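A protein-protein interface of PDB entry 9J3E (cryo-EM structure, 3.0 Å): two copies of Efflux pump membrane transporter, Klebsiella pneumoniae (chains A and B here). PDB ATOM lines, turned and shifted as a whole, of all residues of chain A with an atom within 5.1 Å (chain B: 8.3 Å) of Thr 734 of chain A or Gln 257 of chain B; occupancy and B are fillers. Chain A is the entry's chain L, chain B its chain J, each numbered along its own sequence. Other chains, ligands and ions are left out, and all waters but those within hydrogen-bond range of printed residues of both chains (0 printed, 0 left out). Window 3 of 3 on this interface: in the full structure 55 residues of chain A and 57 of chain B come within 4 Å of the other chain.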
ATOM      1  N   ARG A 729       0.409  15.757   4.751  1.00  0.00           N
ATOM      2  CA  ARG A 729       0.746  16.565   3.585  1.00  0.00           C
ATOM      3  C   ARG A 729      -0.359  17.563   3.276  1.00  0.00           C
ATOM      4  O   ARG A 729      -0.086  18.721   2.944  1.00  0.00           O
ATOM      5  CB  ARG A 729       0.997  15.668   2.376  1.00  0.00           C
ATOM      6  CG  ARG A 729       2.049  14.602   2.588  1.00  0.00           C
ATOM      7  CD  ARG A 729       3.244  14.850   1.693  1.00  0.00           C
ATOM      8  NE  ARG A 729       4.057  13.658   1.496  1.00  0.00           N
ATOM      9  CZ  ARG A 729       4.821  13.445   0.436  1.00  0.00           C
ATOM     10  NH1 ARG A 729       4.911  14.333  -0.539  1.00  0.00           N
ATOM     11  NH2 ARG A 729       5.523  12.321   0.357  1.00  0.00           N
ATOM     12  N   GLU A 730      -1.612  17.131   3.387  1.00  0.00           N
ATOM     13  CA  GLU A 730      -2.736  18.022   3.131  1.00  0.00           C
ATOM     14  C   GLU A 730      -2.778  19.164   4.138  1.00  0.00           C
ATOM     15  O   GLU A 730      -2.947  20.329   3.764  1.00  0.00           O
ATOM     16  CB  GLU A 730      -4.034  17.224   3.169  1.00  0.00           C
ATOM     17  CG  GLU A 730      -3.893  15.784   2.704  1.00  0.00           C
ATOM     18  CD  GLU A 730      -3.300  15.673   1.321  1.00  0.00           C
ATOM     19  OE1 GLU A 730      -3.602  16.544   0.485  1.00  0.00           O
ATOM     20  OE2 GLU A 730      -2.534  14.721   1.071  1.00  0.00           O
ATOM     21  N   GLN A 731      -2.628  18.849   5.426  1.00  0.00           N
ATOM     22  CA  GLN A 731      -2.632  19.897   6.442  1.00  0.00           C
ATOM     23  C   GLN A 731      -1.505  20.889   6.218  1.00  0.00           C
ATOM     24  O   GLN A 731      -1.727  22.103   6.223  1.00  0.00           O
ATOM     25  CB  GLN A 731      -2.506  19.293   7.835  1.00  0.00           C
ATOM     26  CG  GLN A 731      -3.053  20.168   8.926  1.00  0.00           C
ATOM     27  CD  GLN A 731      -3.048  19.477  10.260  1.00  0.00           C
ATOM     28  OE1 GLN A 731      -2.927  18.258  10.335  1.00  0.00           O
ATOM     29  NE2 GLN A 731      -3.160  20.253  11.327  1.00  0.00           N
ATOM     30  N   ALA A 732      -0.290  20.388   6.013  1.00  0.00           N
ATOM     31  CA  ALA A 732       0.834  21.284   5.798  1.00  0.00           C
ATOM     32  C   ALA A 732       0.607  22.137   4.566  1.00  0.00           C
ATOM     33  O   ALA A 732       0.881  23.341   4.577  1.00  0.00           O
ATOM     34  CB  ALA A 732       2.124  20.480   5.666  1.00  0.00           C
ATOM     35  N   ARG A 733       0.086  21.536   3.501  1.00  0.00           N
ATOM     36  CA  ARG A 733      -0.137  22.275   2.268  1.00  0.00           C
ATOM     37  C   ARG A 733      -1.165  23.379   2.457  1.00  0.00           C
ATOM     38  O   ARG A 733      -0.974  24.500   1.976  1.00  0.00           O
ATOM     39  CB  ARG A 733      -0.583  21.314   1.178  1.00  0.00           C
ATOM     40  CG  ARG A 733      -0.605  21.910  -0.195  1.00  0.00           C
ATOM     41  CD  ARG A 733       0.771  22.285  -0.664  1.00  0.00           C
ATOM     42  NE  ARG A 733       0.753  22.531  -2.097  1.00  0.00           N
ATOM     43  CZ  ARG A 733       1.700  23.177  -2.758  1.00  0.00           C
ATOM     44  NH1 ARG A 733       2.753  23.680  -2.138  1.00  0.00           N
ATOM     45  NH2 ARG A 733       1.589  23.320  -4.075  1.00  0.00           N
ATOM     46  N   THR A 734      -2.259  23.082   3.157  1.00  0.00           N
ATOM     47  CA  THR A 734      -3.303  24.080   3.358  1.00  0.00           C
ATOM     48  C   THR A 734      -2.778  25.279   4.128  1.00  0.00           C
ATOM     49  O   THR A 734      -3.085  26.426   3.790  1.00  0.00           O
ATOM     50  CB  THR A 734      -4.492  23.454   4.076  1.00  0.00           C
ATOM     51  OG1 THR A 734      -5.100  22.483   3.218  1.00  0.00           O
ATOM     52  CG2 THR A 734      -5.504  24.506   4.457  1.00  0.00           C
ATOM     53  N   LEU A 735      -1.961  25.040   5.144  1.00  0.00           N
ATOM     54  CA  LEU A 735      -1.300  26.144   5.822  1.00  0.00           C
ATOM     55  C   LEU A 735      -0.318  26.876   4.919  1.00  0.00           C
ATOM     56  O   LEU A 735       0.321  27.827   5.377  1.00  0.00           O
ATOM     57  CB  LEU A 735      -0.576  25.631   7.065  1.00  0.00           C
ATOM     58  CG  LEU A 735      -1.452  24.925   8.095  1.00  0.00           C
ATOM     59  CD1 LEU A 735      -0.594  24.226   9.115  1.00  0.00           C
ATOM     60  CD2 LEU A 735      -2.374  25.898   8.772  1.00  0.00           C
ATOM     61  N   GLY A 736      -0.187  26.470   3.660  1.00  0.00           N
ATOM     62  CA  GLY A 736       0.726  27.121   2.747  1.00  0.00           C
ATOM     63  C   GLY A 736       2.133  26.583   2.766  1.00  0.00           C
ATOM     64  O   GLY A 736       3.042  27.247   2.264  1.00  0.00           O
ATOM     65  N   ASP A 790       3.517  30.091   2.280  1.00  0.00           N
ATOM     66  CA  ASP A 790       3.571  30.955   1.108  1.00  0.00           C
ATOM     67  C   ASP A 790       3.383  32.423   1.471  1.00  0.00           C
ATOM     68  O   ASP A 790       3.823  33.305   0.728  1.00  0.00           O
ATOM     69  CB  ASP A 790       2.544  30.503   0.067  1.00  0.00           C
ATOM     70  CG  ASP A 790       1.114  30.844   0.444  1.00  0.00           C
ATOM     71  OD1 ASP A 790       0.863  31.347   1.558  1.00  0.00           O
ATOM     72  OD2 ASP A 790       0.223  30.606  -0.397  1.00  0.00           O
ATOM     73  N   VAL B 252      -0.799  17.141  -4.078  1.00  0.00           N
ATOM     74  CA  VAL B 252      -1.605  18.353  -4.019  1.00  0.00           C
ATOM     75  C   VAL B 252      -1.078  19.336  -5.050  1.00  0.00           C
ATOM     76  O   VAL B 252       0.076  19.766  -4.974  1.00  0.00           O
ATOM     77  CB  VAL B 252      -1.576  18.967  -2.617  1.00  0.00           C
ATOM     78  CG1 VAL B 252      -2.608  20.059  -2.509  1.00  0.00           C
ATOM     79  CG2 VAL B 252      -1.802  17.901  -1.585  1.00  0.00           C
ATOM     80  N   ARG B 254      -2.890  22.342  -5.868  1.00  0.00           N
ATOM     81  CA  ARG B 254      -3.188  23.664  -5.341  1.00  0.00           C
ATOM     82  C   ARG B 254      -4.195  23.515  -4.216  1.00  0.00           C
ATOM     83  O   ARG B 254      -5.287  22.983  -4.423  1.00  0.00           O
ATOM     84  CB  ARG B 254      -3.725  24.580  -6.439  1.00  0.00           C
ATOM     85  CG  ARG B 254      -4.703  25.631  -5.977  1.00  0.00           C
ATOM     86  CD  ARG B 254      -4.673  26.811  -6.924  1.00  0.00           C
ATOM     87  NE  ARG B 254      -5.731  26.719  -7.920  1.00  0.00           N
ATOM     88  CZ  ARG B 254      -5.530  26.785  -9.229  1.00  0.00           C
ATOM     89  NH1 ARG B 254      -4.322  26.969  -9.733  1.00  0.00           N
ATOM     90  NH2 ARG B 254      -6.567  26.659 -10.051  1.00  0.00           N
ATOM     91  N   ALA B 255      -3.823  23.979  -3.033  1.00  0.00           N
ATOM     92  CA  ALA B 255      -4.672  23.866  -1.863  1.00  0.00           C
ATOM     93  C   ALA B 255      -4.918  25.254  -1.305  1.00  0.00           C
ATOM     94  O   ALA B 255      -4.001  26.075  -1.233  1.00  0.00           O
ATOM     95  CB  ALA B 255      -4.042  22.975  -0.794  1.00  0.00           C
ATOM     96  N   ASN B 256      -6.160  25.510  -0.922  1.00  0.00           N
ATOM     97  CA  ASN B 256      -6.560  26.794  -0.376  1.00  0.00           C
ATOM     98  C   ASN B 256      -6.510  26.757   1.141  1.00  0.00           C
ATOM     99  O   ASN B 256      -6.416  25.698   1.761  1.00  0.00           O
ATOM    100  CB  ASN B 256      -7.965  27.158  -0.852  1.00  0.00           C
ATOM    101  CG  ASN B 256      -7.990  27.571  -2.294  1.00  0.00           C
ATOM    102  OD1 ASN B 256      -7.039  28.165  -2.794  1.00  0.00           O
ATOM    103  ND2 ASN B 256      -9.076  27.254  -2.982  1.00  0.00           N
ATOM    104  N   GLN B 257      -6.580  27.943   1.742  1.00  0.00           N
ATOM    105  CA  GLN B 257      -6.591  28.024   3.195  1.00  0.00           C
ATOM    106  C   GLN B 257      -7.850  27.408   3.781  1.00  0.00           C
ATOM    107  O   GLN B 257      -7.806  26.846   4.879  1.00  0.00           O
ATOM    108  CB  GLN B 257      -6.465  29.475   3.640  1.00  0.00           C
ATOM    109  CG  GLN B 257      -5.254  30.183   3.091  1.00  0.00           C
ATOM    110  CD  GLN B 257      -4.316  30.630   4.184  1.00  0.00           C
ATOM    111  OE1 GLN B 257      -4.736  30.870   5.311  1.00  0.00           O
ATOM    112  NE2 GLN B 257      -3.038  30.756   3.855  1.00  0.00           N
ATOM    113  N   ASP B 258      -8.973  27.501   3.070  1.00  0.00           N
ATOM    114  CA  ASP B 258     -10.218  26.951   3.591  1.00  0.00           C
ATOM    115  C   ASP B 258     -10.110  25.449   3.799  1.00  0.00           C
ATOM    116  O   ASP B 258     -10.608  24.916   4.796  1.00  0.00           O
ATOM    117  CB  ASP B 258     -11.375  27.286   2.650  1.00  0.00           C
ATOM    118  CG  ASP B 258     -11.218  26.659   1.278  1.00  0.00           C
ATOM    119  OD1 ASP B 258     -11.315  25.419   1.160  1.00  0.00           O
ATOM    120  OD2 ASP B 258     -11.003  27.412   0.309  1.00  0.00           O
ATOM    121  N   GLY B 259      -9.456  24.753   2.877  1.00  0.00           N
ATOM    122  CA  GLY B 259      -9.324  23.316   2.966  1.00  0.00           C
ATOM    123  C   GLY B 259      -9.435  22.640   1.618  1.00  0.00           C
ATOM    124  O   GLY B 259      -8.925  21.535   1.430  1.00  0.00           O
ATOM    125  N   SER B 260     -10.090  23.300   0.669  1.00  0.00           N
ATOM    126  CA  SER B 260     -10.233  22.731  -0.662  1.00  0.00           C
ATOM    127  C   SER B 260      -8.867  22.523  -1.297  1.00  0.00           C
ATOM    128  O   SER B 260      -7.979  23.371  -1.192  1.00  0.00           O
ATOM    129  CB  SER B 260     -11.081  23.640  -1.544  1.00  0.00           C
ATOM    130  OG  SER B 260     -11.251  23.067  -2.828  1.00  0.00           O
ATOM    131  N   ARG B 261      -8.699  21.383  -1.956  1.00  0.00           N
ATOM    132  CA  ARG B 261      -7.427  21.021  -2.554  1.00  0.00           C
ATOM    133  C   ARG B 261      -7.632  20.485  -3.958  1.00  0.00           C
ATOM    134  O   ARG B 261      -8.706  19.988  -4.298  1.00  0.00           O
ATOM    135  CB  ARG B 261      -6.700  19.979  -1.720  1.00  0.00           C
ATOM    136  CG  ARG B 261      -7.252  18.584  -1.872  1.00  0.00           C
ATOM    137  CD  ARG B 261      -6.579  17.580  -0.953  1.00  0.00           C
ATOM    138  NE  ARG B 261      -6.978  17.723   0.441  1.00  0.00           N
ATOM    139  CZ  ARG B 261      -6.426  18.568   1.301  1.00  0.00           C
ATOM    140  NH1 ARG B 261      -5.397  19.325   0.965  1.00  0.00           N
ATOM    141  NH2 ARG B 261      -6.898  18.631   2.541  1.00  0.00           N
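The guanidinium group of Arg 261 of chain B lies within salt-bridge range of the side-chain carboxylate of Glu 730 of chain A (3.3 Å).
The backbone carbonyl oxygen (O) of Glu 730 of chain A is in hydrogen-bond range of the side-chain hydroxyl (OG1) of Thr 734 of chain A (3.1 Å).
Among the printed residues, merely in contact across the chains: Glu 730 of chain A with Val 252 of chain B (3.1 Å), Thr 734 of chain A with Asn 256 of chain B (3.1 Å), Thr 734 of chain A with Gln 257 of chain B (3.3 Å), Arg 733 of chain A with Val 252 of chain B (3.6 Å), Arg 733 of chain A with Ala 255 of chain B (3.6 Å) and Thr 734 of chain A with Arg 261 of chain B (3.9 Å).
Printed residues of chain B within 4 Å of Glu 730 of chain A: Val 252 and Arg 261. Of the printed residues of chain B, Arg 733 of chain A touches Val 252 (3.6 Å) and Ala 255 (3.6 Å). Of chain B, only Asn 256 (3.1 Å), Gln 257 (3.3 Å) and Arg 261 (3.9 Å) come within 4 Å of Thr 734 of chain A. Gly 736 of chain A touches none of the printed residues of chain B. Asp 790 of chain A touches none of the printed residues of chain B. Of the printed residues of chain A, Val 252 of chain B touches Glu 730 and Arg 733. Printed residues of chain A within 4 Å of Ala 255 of chain B: Arg 733. Printed residues of chain A within 4 Å of Asn 256 of chain B: Thr 734. Gln 257 of chain B touches just one residue of chain A: Thr 734 (3.3 Å). The nearest residue of chain A that does not touch Gln 257 of chain B is Asp 790 of chain A (4.6 Å). The nearest printed residue of chain A that does not touch Asn 256 of chain B is Arg 733 of chain A (5.6 Å).
Printed residues of chain B that touch a printed residue of chain A: Val 252, Ala 255, Asn 256, Gln 257 and Arg 261. Of the 9 printed residues of chain A, 3 touch a printed residue of chain B. Printed residues of chain A that touch a printed residue of chain B: Glu 730, Arg 733 and Thr 734. Among the printed residues, 7 pairs touch across the chains.
No position is printed for both chains. Of the 7 pairs that touch across the chains among the printed residues, none has its exchanged pair printed and touching as well.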
